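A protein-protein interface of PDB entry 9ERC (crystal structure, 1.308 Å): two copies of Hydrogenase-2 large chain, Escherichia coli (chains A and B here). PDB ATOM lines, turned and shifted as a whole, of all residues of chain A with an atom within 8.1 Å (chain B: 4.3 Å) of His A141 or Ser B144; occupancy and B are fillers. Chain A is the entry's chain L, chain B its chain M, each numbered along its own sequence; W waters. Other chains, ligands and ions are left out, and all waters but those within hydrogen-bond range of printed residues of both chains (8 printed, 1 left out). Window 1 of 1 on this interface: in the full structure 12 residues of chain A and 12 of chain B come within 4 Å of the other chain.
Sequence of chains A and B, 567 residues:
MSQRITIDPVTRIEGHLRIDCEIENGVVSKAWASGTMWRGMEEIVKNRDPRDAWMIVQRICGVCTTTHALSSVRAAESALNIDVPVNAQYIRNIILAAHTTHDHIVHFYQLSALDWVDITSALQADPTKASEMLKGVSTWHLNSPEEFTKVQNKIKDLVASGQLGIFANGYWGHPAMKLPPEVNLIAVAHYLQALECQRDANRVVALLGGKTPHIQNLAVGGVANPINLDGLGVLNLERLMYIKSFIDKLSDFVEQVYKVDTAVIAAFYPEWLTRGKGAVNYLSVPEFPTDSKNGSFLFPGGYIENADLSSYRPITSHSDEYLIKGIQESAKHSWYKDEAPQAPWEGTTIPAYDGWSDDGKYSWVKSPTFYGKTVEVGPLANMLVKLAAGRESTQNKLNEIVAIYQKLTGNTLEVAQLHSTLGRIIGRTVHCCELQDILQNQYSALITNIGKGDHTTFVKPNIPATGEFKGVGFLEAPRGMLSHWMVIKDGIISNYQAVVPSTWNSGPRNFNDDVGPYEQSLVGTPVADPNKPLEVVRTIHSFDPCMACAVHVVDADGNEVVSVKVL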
ATOM      1  N   SER A 131      -7.366 -22.560   3.738  1.00  0.00           N
ATOM      2  CA  SER A 131      -7.002 -22.267   2.366  1.00  0.00           C
ATOM      3  C   SER A 131      -8.168 -22.531   1.401  1.00  0.00           C
ATOM      4  O   SER A 131      -8.415 -21.757   0.474  1.00  0.00           O
ATOM      5  CB  SER A 131      -5.738 -23.038   1.988  1.00  0.00           C
ATOM      6  OG  SER A 131      -5.334 -22.716   0.677  1.00  0.00           O
ATOM      7  N   LYS A 135     -10.906 -20.301  -2.049  1.00  0.00           N
ATOM      8  CA  LYS A 135     -10.957 -20.615  -3.475  1.00  0.00           C
ATOM      9  C   LYS A 135     -12.107 -19.871  -4.138  1.00  0.00           C
ATOM     10  O   LYS A 135     -13.196 -19.829  -3.583  1.00  0.00           O
ATOM     11  CB  LYS A 135     -11.156 -22.117  -3.644  1.00  0.00           C
ATOM     12  CG  LYS A 135     -10.037 -22.963  -3.081  1.00  0.00           C
ATOM     13  CD  LYS A 135      -8.741 -22.801  -3.830  1.00  0.00           C
ATOM     14  CE  LYS A 135      -7.575 -23.413  -3.084  1.00  0.00           C
ATOM     15  NZ  LYS A 135      -6.285 -22.999  -3.665  1.00  0.00           N
ATOM     16  N   SER A 138     -10.317 -15.252  -3.695  1.00  0.00           N
ATOM     17  CA  SER A 138      -9.070 -14.514  -3.859  1.00  0.00           C
ATOM     18  C   SER A 138      -8.137 -15.278  -4.785  1.00  0.00           C
ATOM     19  O   SER A 138      -8.152 -16.504  -4.761  1.00  0.00           O
ATOM     20  CB  SER A 138      -8.374 -14.310  -2.538  1.00  0.00           C
ATOM     21  OG  SER A 138      -7.146 -13.621  -2.734  1.00  0.00           O
ATOM     22  N   THR A 139      -7.301 -14.535  -5.497  1.00  0.00           N
ATOM     23  CA  THR A 139      -6.211 -15.073  -6.286  1.00  0.00           C
ATOM     24  C   THR A 139      -4.852 -14.817  -5.627  1.00  0.00           C
ATOM     25  O   THR A 139      -3.813 -15.048  -6.261  1.00  0.00           O
ATOM     26  CB  THR A 139      -6.207 -14.472  -7.695  1.00  0.00           C
ATOM     27  OG1 THR A 139      -6.051 -13.061  -7.594  1.00  0.00           O
ATOM     28  CG2 THR A 139      -7.486 -14.798  -8.440  1.00  0.00           C
ATOM     29  N   TRP A 140      -4.844 -14.366  -4.363  1.00  0.00           N
ATOM     30  CA  TRP A 140      -3.602 -14.107  -3.643  1.00  0.00           C
ATOM     31  C   TRP A 140      -2.757 -15.372  -3.589  1.00  0.00           C
ATOM     32  O   TRP A 140      -3.275 -16.450  -3.301  1.00  0.00           O
ATOM     33  CB  TRP A 140      -3.917 -13.636  -2.233  1.00  0.00           C
ATOM     34  CG  TRP A 140      -2.773 -13.300  -1.338  1.00  0.00           C
ATOM     35  CD1 TRP A 140      -2.556 -13.796  -0.088  1.00  0.00           C
ATOM     36  CD2 TRP A 140      -1.761 -12.289  -1.540  1.00  0.00           C
ATOM     37  NE1 TRP A 140      -1.502 -13.161   0.507  1.00  0.00           N
ATOM     38  CE2 TRP A 140      -0.971 -12.266  -0.361  1.00  0.00           C
ATOM     39  CE3 TRP A 140      -1.454 -11.408  -2.589  1.00  0.00           C
ATOM     40  CZ2 TRP A 140       0.088 -11.377  -0.204  1.00  0.00           C
ATOM     41  CZ3 TRP A 140      -0.396 -10.538  -2.432  1.00  0.00           C
ATOM     42  CH2 TRP A 140       0.363 -10.536  -1.258  1.00  0.00           C
ATOM     43  N   HIS A 141      -1.444 -15.172  -3.776  1.00  0.00           N
ATOM     44  CA  HIS A 141      -0.470 -16.243  -3.866  1.00  0.00           C
ATOM     45  C   HIS A 141       0.041 -16.753  -2.520  1.00  0.00           C
ATOM     46  O   HIS A 141       0.792 -17.707  -2.505  1.00  0.00           O
ATOM     47  CB  HIS A 141       0.688 -15.790  -4.759  1.00  0.00           C
ATOM     48  CG  HIS A 141       1.614 -14.759  -4.180  1.00  0.00           C
ATOM     49  ND1 HIS A 141       2.952 -14.705  -4.516  1.00  0.00           N
ATOM     50  CD2 HIS A 141       1.414 -13.714  -3.380  1.00  0.00           C
ATOM     51  CE1 HIS A 141       3.524 -13.675  -3.894  1.00  0.00           C
ATOM     52  NE2 HIS A 141       2.615 -13.098  -3.150  1.00  0.00           N
ATOM     53  N   LEU A 142      -0.366 -16.164  -1.382  1.00  0.00           N
ATOM     54  CA  LEU A 142       0.140 -16.550  -0.065  1.00  0.00           C
ATOM     55  C   LEU A 142      -0.993 -16.941   0.884  1.00  0.00           C
ATOM     56  O   LEU A 142      -1.003 -16.610   2.069  1.00  0.00           O
ATOM     57  CB  LEU A 142       0.961 -15.376   0.479  1.00  0.00           C
ATOM     58  CG  LEU A 142       2.427 -15.357   0.080  1.00  0.00           C
ATOM     59  CD1 LEU A 142       3.101 -14.050   0.476  1.00  0.00           C
ATOM     60  CD2 LEU A 142       3.154 -16.505   0.726  1.00  0.00           C
ATOM     61  N   ASN A 143      -1.917 -17.741   0.337  1.00  0.00           N
ATOM     62  CA  ASN A 143      -3.014 -18.328   1.086  1.00  0.00           C
ATOM     63  C   ASN A 143      -2.916 -19.857   1.141  1.00  0.00           C
ATOM     64  O   ASN A 143      -3.916 -20.526   1.396  1.00  0.00           O
ATOM     65  CB  ASN A 143      -4.344 -17.899   0.462  1.00  0.00           C
ATOM     66  CG  ASN A 143      -4.747 -16.491   0.858  1.00  0.00           C
ATOM     67  OD1 ASN A 143      -4.448 -16.042   1.951  1.00  0.00           O
ATOM     68  ND2 ASN A 143      -5.522 -15.857   0.011  1.00  0.00           N
ATOM     69  N   SER A 144      -1.705 -20.425   0.980  1.00  0.00           N
ATOM     70  CA  SER A 144      -1.577 -21.874   0.985  1.00  0.00           C
ATOM     71  C   SER A 144      -1.756 -22.421   2.380  1.00  0.00           C
ATOM     72  O   SER A 144      -1.514 -21.753   3.377  1.00  0.00           O
ATOM     73  CB  SER A 144      -0.235 -22.318   0.448  1.00  0.00           C
ATOM     74  OG  SER A 144       0.790 -21.874   1.303  1.00  0.00           O
ATOM     75  N   PRO A 145      -2.123 -23.720   2.506  1.00  0.00           N
ATOM     76  CA  PRO A 145      -2.083 -24.384   3.802  1.00  0.00           C
ATOM     77  C   PRO A 145      -0.718 -24.284   4.464  1.00  0.00           C
ATOM     78  O   PRO A 145      -0.652 -24.181   5.674  1.00  0.00           O
ATOM     79  CB  PRO A 145      -2.492 -25.830   3.477  1.00  0.00           C
ATOM     80  CG  PRO A 145      -3.228 -25.742   2.188  1.00  0.00           C
ATOM     81  CD  PRO A 145      -2.583 -24.608   1.421  1.00  0.00           C
ATOM     82  N   GLU A 146       0.344 -24.297   3.656  1.00  0.00           N
ATOM     83  CA  GLU A 146       1.691 -24.275   4.192  1.00  0.00           C
ATOM     84  C   GLU A 146       2.010 -22.901   4.797  1.00  0.00           C
ATOM     85  O   GLU A 146       2.611 -22.813   5.874  1.00  0.00           O
ATOM     86  CB  GLU A 146       2.681 -24.591   3.070  1.00  0.00           C
ATOM     87  CG  GLU A 146       2.648 -26.037   2.604  1.00  0.00           C
ATOM     88  CD  GLU A 146       1.477 -26.469   1.732  1.00  0.00           C
ATOM     89  OE1 GLU A 146       0.727 -25.611   1.186  1.00  0.00           O
ATOM     90  OE2 GLU A 146       1.349 -27.711   1.526  1.00  0.00           O
ATOM     91  N   GLU A 147       1.563 -21.835   4.130  1.00  0.00           N
ATOM     92  CA  GLU A 147       1.684 -20.494   4.710  1.00  0.00           C
ATOM     93  C   GLU A 147       0.936 -20.440   6.038  1.00  0.00           C
ATOM     94  O   GLU A 147       1.453 -19.965   7.051  1.00  0.00           O
ATOM     95  CB  GLU A 147       1.140 -19.437   3.759  1.00  0.00           C
ATOM     96  CG  GLU A 147       1.092 -18.036   4.363  1.00  0.00           C
ATOM     97  CD  GLU A 147       2.426 -17.344   4.628  1.00  0.00           C
ATOM     98  OE1 GLU A 147       3.493 -17.986   4.454  1.00  0.00           O
ATOM     99  OE2 GLU A 147       2.393 -16.131   5.002  1.00  0.00           O
ATOM    100  N   GLN A 193       1.328 -10.512   6.793  1.00  0.00           N
ATOM    101  CA  GLN A 193       1.638 -10.148   5.413  1.00  0.00           C
ATOM    102  C   GLN A 193       1.464  -8.651   5.163  1.00  0.00           C
ATOM    103  O   GLN A 193       2.193  -8.059   4.367  1.00  0.00           O
ATOM    104  CB  GLN A 193       0.784 -10.959   4.436  1.00  0.00           C
ATOM    105  CG  GLN A 193       1.142 -12.437   4.471  1.00  0.00           C
ATOM    106  CD  GLN A 193       0.067 -13.282   3.837  1.00  0.00           C
ATOM    107  OE1 GLN A 193      -0.846 -12.781   3.194  1.00  0.00           O
ATOM    108  NE2 GLN A 193       0.214 -14.586   4.001  1.00  0.00           N
ATOM    109  N   ASP A 252      -1.359  -5.908  -5.459  1.00  0.00           N
ATOM    110  CA  ASP A 252      -1.880  -7.256  -5.297  1.00  0.00           C
ATOM    111  C   ASP A 252      -2.377  -7.492  -3.868  1.00  0.00           C
ATOM    112  O   ASP A 252      -3.448  -8.076  -3.678  1.00  0.00           O
ATOM    113  CB  ASP A 252      -0.839  -8.321  -5.643  1.00  0.00           C
ATOM    114  CG  ASP A 252      -0.570  -8.464  -7.126  1.00  0.00           C
ATOM    115  OD1 ASP A 252      -1.273  -7.845  -7.934  1.00  0.00           O
ATOM    116  OD2 ASP A 252       0.341  -9.257  -7.437  1.00  0.00           O
ATOM    117  N   PHE A 253      -1.618  -7.056  -2.854  1.00  0.00           N
ATOM    118  CA  PHE A 253      -2.059  -7.242  -1.480  1.00  0.00           C
ATOM    119  C   PHE A 253      -3.360  -6.468  -1.266  1.00  0.00           C
ATOM    120  O   PHE A 253      -4.305  -6.952  -0.640  1.00  0.00           O
ATOM    121  CB  PHE A 253      -0.993  -6.816  -0.470  1.00  0.00           C
ATOM    122  CG  PHE A 253      -1.425  -6.970   0.964  1.00  0.00           C
ATOM    123  CD1 PHE A 253      -2.113  -5.962   1.618  1.00  0.00           C
ATOM    124  CD2 PHE A 253      -1.220  -8.158   1.645  1.00  0.00           C
ATOM    125  CE1 PHE A 253      -2.577  -6.159   2.910  1.00  0.00           C
ATOM    126  CE2 PHE A 253      -1.669  -8.342   2.943  1.00  0.00           C
ATOM    127  CZ  PHE A 253      -2.380  -7.338   3.566  1.00  0.00           C
ATOM    128  N   GLN A 256      -6.215  -8.292  -3.379  1.00  0.00           N
ATOM    129  CA  GLN A 256      -6.456  -9.727  -3.227  1.00  0.00           C
ATOM    130  C   GLN A 256      -6.490 -10.139  -1.761  1.00  0.00           C
ATOM    131  O   GLN A 256      -6.838 -11.286  -1.459  1.00  0.00           O
ATOM    132  CB  GLN A 256      -5.370 -10.501  -3.997  1.00  0.00           C
ATOM    133  CG  GLN A 256      -5.297 -10.181  -5.484  1.00  0.00           C
ATOM    134  CD  GLN A 256      -4.032 -10.684  -6.157  1.00  0.00           C
ATOM    135  OE1 GLN A 256      -3.202 -11.382  -5.577  1.00  0.00           O
ATOM    136  NE2 GLN A 256      -3.822 -10.296  -7.406  1.00  0.00           N
ATOM    137  N   VAL A 257      -6.090  -9.228  -0.836  1.00  0.00           N
ATOM    138  CA  VAL A 257      -6.052  -9.561   0.578  1.00  0.00           C
ATOM    139  C   VAL A 257      -6.925  -8.581   1.350  1.00  0.00           C
ATOM    140  O   VAL A 257      -7.939  -8.971   1.926  1.00  0.00           O
ATOM    141  CB  VAL A 257      -4.629  -9.638   1.159  1.00  0.00           C
ATOM    142  CG1 VAL A 257      -4.656 -10.124   2.595  1.00  0.00           C
ATOM    143  CG2 VAL A 257      -3.743 -10.532   0.317  1.00  0.00           C
ATOM    144  N   SER B 131       0.207 -28.126  -7.402  1.00  0.00           N
ATOM    145  CA  SER B 131       0.331 -27.887  -5.979  1.00  0.00           C
ATOM    146  C   SER B 131       0.137 -29.172  -5.168  1.00  0.00           C
ATOM    147  O   SER B 131       0.856 -29.437  -4.204  1.00  0.00           O
ATOM    148  CB  SER B 131      -0.628 -26.770  -5.568  1.00  0.00           C
ATOM    149  OG  SER B 131      -0.502 -26.515  -4.183  1.00  0.00           O
ATOM    150  N   LEU B 142       5.088 -21.022  -0.881  1.00  0.00           N
ATOM    151  CA  LEU B 142       4.754 -20.410  -2.168  1.00  0.00           C
ATOM    152  C   LEU B 142       4.599 -21.463  -3.283  1.00  0.00           C
ATOM    153  O   LEU B 142       5.054 -21.286  -4.425  1.00  0.00           O
ATOM    154  CB  LEU B 142       5.849 -19.391  -2.485  1.00  0.00           C
ATOM    155  CG  LEU B 142       5.586 -17.992  -1.942  1.00  0.00           C
ATOM    156  CD1 LEU B 142       6.821 -17.106  -2.123  1.00  0.00           C
ATOM    157  CD2 LEU B 142       4.385 -17.377  -2.654  1.00  0.00           C
ATOM    158  N   ASN B 143       3.893 -22.545  -2.925  1.00  0.00           N
ATOM    159  CA  ASN B 143       3.538 -23.592  -3.875  1.00  0.00           C
ATOM    160  C   ASN B 143       2.022 -23.698  -4.071  1.00  0.00           C
ATOM    161  O   ASN B 143       1.526 -24.744  -4.488  1.00  0.00           O
ATOM    162  CB  ASN B 143       4.072 -24.932  -3.394  1.00  0.00           C
ATOM    163  CG  ASN B 143       5.559 -25.104  -3.647  1.00  0.00           C
ATOM    164  OD1 ASN B 143       6.067 -24.610  -4.657  1.00  0.00           O
ATOM    165  ND2 ASN B 143       6.175 -25.895  -2.793  1.00  0.00           N
ATOM    166  N   SER B 144       1.275 -22.618  -3.822  1.00  0.00           N
ATOM    167  CA  SER B 144      -0.162 -22.666  -3.995  1.00  0.00           C
ATOM    168  C   SER B 144      -0.531 -22.751  -5.467  1.00  0.00           C
ATOM    169  O   SER B 144       0.183 -22.265  -6.333  1.00  0.00           O
ATOM    170  CB  SER B 144      -0.810 -21.431  -3.404  1.00  0.00           C
ATOM    171  OG  SER B 144      -0.407 -20.269  -4.113  1.00  0.00           O
ATOM    172  N   PRO B 145      -1.751 -23.251  -5.770  1.00  0.00           N
ATOM    173  CA  PRO B 145      -2.294 -23.147  -7.118  1.00  0.00           C
ATOM    174  C   PRO B 145      -2.309 -21.711  -7.623  1.00  0.00           C
ATOM    175  O   PRO B 145      -2.109 -21.450  -8.797  1.00  0.00           O
ATOM    176  CB  PRO B 145      -3.710 -23.751  -6.993  1.00  0.00           C
ATOM    177  CG  PRO B 145      -3.651 -24.628  -5.746  1.00  0.00           C
ATOM    178  CD  PRO B 145      -2.651 -23.940  -4.839  1.00  0.00           C
ATOM    179  N   GLU B 146      -2.545 -20.760  -6.716  1.00  0.00           N
ATOM    180  CA  GLU B 146      -2.630 -19.360  -7.099  1.00  0.00           C
ATOM    181  C   GLU B 146      -1.269 -18.806  -7.526  1.00  0.00           C
ATOM    182  O   GLU B 146      -1.170 -18.072  -8.504  1.00  0.00           O
ATOM    183  CB  GLU B 146      -3.219 -18.543  -5.944  1.00  0.00           C
ATOM    184  CG  GLU B 146      -4.700 -18.861  -5.705  1.00  0.00           C
ATOM    185  CD  GLU B 146      -5.032 -20.157  -4.961  1.00  0.00           C
ATOM    186  OE1 GLU B 146      -4.126 -20.798  -4.365  1.00  0.00           O
ATOM    187  OE2 GLU B 146      -6.229 -20.518  -4.923  1.00  0.00           O
ATOM    188  N   GLU B 147      -0.208 -19.161  -6.786  1.00  0.00           N
ATOM    189  CA  GLU B 147       1.129 -18.808  -7.229  1.00  0.00           C
ATOM    190  C   GLU B 147       1.399 -19.402  -8.604  1.00  0.00           C
ATOM    191  O   GLU B 147       1.907 -18.739  -9.504  1.00  0.00           O
ATOM    192  CB  GLU B 147       2.150 -19.332  -6.221  1.00  0.00           C
ATOM    193  CG  GLU B 147       3.593 -19.120  -6.646  1.00  0.00           C
ATOM    194  CD  GLU B 147       4.129 -17.686  -6.699  1.00  0.00           C
ATOM    195  OE1 GLU B 147       3.361 -16.700  -6.519  1.00  0.00           O
ATOM    196  OE2 GLU B 147       5.349 -17.532  -6.904  1.00  0.00           O
ATOM    197  N   PHE B 148       1.084 -20.685  -8.755  1.00  0.00           N
ATOM    198  CA  PHE B 148       1.375 -21.378 -10.006  1.00  0.00           C
ATOM    199  C   PHE B 148       0.589 -20.818 -11.179  1.00  0.00           C
ATOM    200  O   PHE B 148       1.092 -20.790 -12.284  1.00  0.00           O
ATOM    201  CB  PHE B 148       1.163 -22.879  -9.845  1.00  0.00           C
ATOM    202  CG  PHE B 148       2.138 -23.564  -8.920  1.00  0.00           C
ATOM    203  CD1 PHE B 148       3.338 -22.963  -8.521  1.00  0.00           C
ATOM    204  CD2 PHE B 148       1.862 -24.828  -8.440  1.00  0.00           C
ATOM    205  CE1 PHE B 148       4.226 -23.633  -7.699  1.00  0.00           C
ATOM    206  CE2 PHE B 148       2.755 -25.494  -7.612  1.00  0.00           C
ATOM    207  CZ  PHE B 148       3.944 -24.900  -7.236  1.00  0.00           C
ATOM    208  N   LYS B 150      -0.354 -17.596 -11.410  1.00  0.00           N
ATOM    209  CA  LYS B 150       0.312 -16.327 -11.710  1.00  0.00           C
ATOM    210  C   LYS B 150       1.505 -16.581 -12.658  1.00  0.00           C
ATOM    211  O   LYS B 150       1.714 -15.891 -13.668  1.00  0.00           O
ATOM    212  CB  LYS B 150       0.720 -15.577 -10.412  1.00  0.00           C
ATOM    213  CG  LYS B 150      -0.413 -14.964  -9.553  1.00  0.00           C
ATOM    214  CD  LYS B 150      -0.035 -14.055  -8.291  1.00  0.00           C
ATOM    215  CE  LYS B 150      -1.195 -13.435  -7.469  1.00  0.00           C
ATOM    216  NZ  LYS B 150      -0.864 -12.815  -6.097  1.00  0.00           N
HETATM  217  O   HOH W   1       1.378 -10.960  -5.767  1.00  0.00           O
HETATM  218  O   HOH W   2       6.090 -15.267  -5.811  1.00  0.00           O
HETATM  219  O   HOH W   3       1.123 -19.986  -1.179  1.00  0.00           O
HETATM  220  O   HOH W   4      -7.697 -18.863  -3.147  1.00  0.00           O
HETATM  221  O   HOH W   5       0.801 -25.323  -1.346  1.00  0.00           O
HETATM  222  O   HOH W   6      -3.379 -16.382  -8.809  1.00  0.00           O
HETATM  223  O   HOH W   7      -4.005 -20.912  -1.825  1.00  0.00           O
HETATM  224  O   HOH W   8       2.650 -23.343  -0.394  1.00  0.00           O
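His A141 touches just these residues of chain B: Leu B142, Ser B144, Glu B147 and Lys B150.
Of the printed residues of chain B, Asp A252 touches Lys B150.
Printed residues of chain B within 4 Å of Gln A256: Lys B150 (2.8 Å).
Of the printed residues of chain A, Ser B144 touches His A141 and Ser A144.
Pro B145 touches one residue of chain A.
The nearest printed residue of chain A that does not touch Ser B144 is Trp A140 (4.8 Å).
Leu B142 touches its own counterpart, Leu A142.
Ser A144 touches its own counterpart, Ser B144.
Of the 14 pairs that touch across the chains among the printed residues, 2 have their exchanged pair printed and touching as well.
Among the printed residues, pairs that only touch across the chains: Lys A135 with Pro B145 (3.7 Å), Thr A139 with Glu B146 (3.6 Å), Thr A139 with Lys B150 (3.3 Å), Trp A140 with Glu B146 (3.4 Å), Trp A140 with Lys B150 (3.8 Å), His A141 with Leu B142 (3.6 Å), Leu A142 with Leu B142 (3.7 Å) and Ser A144 with Ser B144 (3.99 Å).
The backbone carbonyl oxygen (O) of His A141 is in hydrogen-bond range of the side-chain hydroxyl (OG) of Ser B144 (3.3 Å).
The backbone NH (N) of His A141 sits close to the side-chain amino group (NZ) of Lys B150 (3.4 Å).
NZ of Lys A135 lies within salt-bridge range of OE2 of Glu B146 (2.8 Å).
The side-chain amide oxygen (OE1) of Gln A256 is in hydrogen-bond range of the side-chain amino group (NZ) of Lys B150 (2.8 Å).
ND1 of His A141 is in hydrogen-bond range of OE1 of Glu B147 (2.9 Å).
The side-chain carboxylate of Asp A252 lies within salt-bridge range of the side-chain amino group of Lys B150, 3.99 Å away.
Hydrophobic or aromatic side chains of chain A within 4 Å of the printed part of chain B: Trp A140, His A141 and Leu A142.
Among the printed residues, Asp or Glu carboxylates within 4 Å of a Lys or Arg side-chain nitrogen of the other chain: Lys A135 with Glu B146 (2.8 Å) and Asp A252 with Lys B150 (3.99 Å).
Water W5 lies within hydrogen-bond range of OE1 of Glu A146, O of Asn B143 and OG of Ser B131.
Water W2 bridges OE2 of Glu B147 (2.6 Å) and ND1 of His A141 (3.4 Å).
Water W3 lies within hydrogen-bond range of O of His A141, OG of Ser A144 and OG of Ser B144.
Water W6 lies within hydrogen-bond range of the backbone carbonyl oxygen of Glu B146 (2.8 Å) and the backbone carbonyl oxygen of Thr A139 (2.9 Å).
Water W4 bridges the side-chain carboxylate of Glu B146 (2.8 Å) and the backbone carbonyl oxygen of Ser A138 (2.9 Å).
Water W8 lies within hydrogen-bond range of the side-chain hydroxyl of Ser A144 (2.9 Å), the backbone NH of Asn B143 (2.9 Å), the side-chain carboxylate of Glu A146 (3.4 Å) and the backbone NH of Leu B142 (3.4 Å).
O of Gln A256 is in hydrogen-bond range of OG of Ser A138 (2.7 Å).
The backbone NH (N) of Glu A146 lies close to the side-chain hydroxyl (OG) of Ser A144 (3.4 Å).
OG of Ser A138 sits at hydrogen-bond distance from N of Trp A140 (2.9 Å).
NE2 of Gln A193 lies within hydrogen-bond range of O of Leu A142, 3.1 Å away.
OG of Ser B144 sits at hydrogen-bond distance from N of Glu B147, at 2.9 Å.
OG of Ser B144 sits close to N of Glu B146 (3.4 Å).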
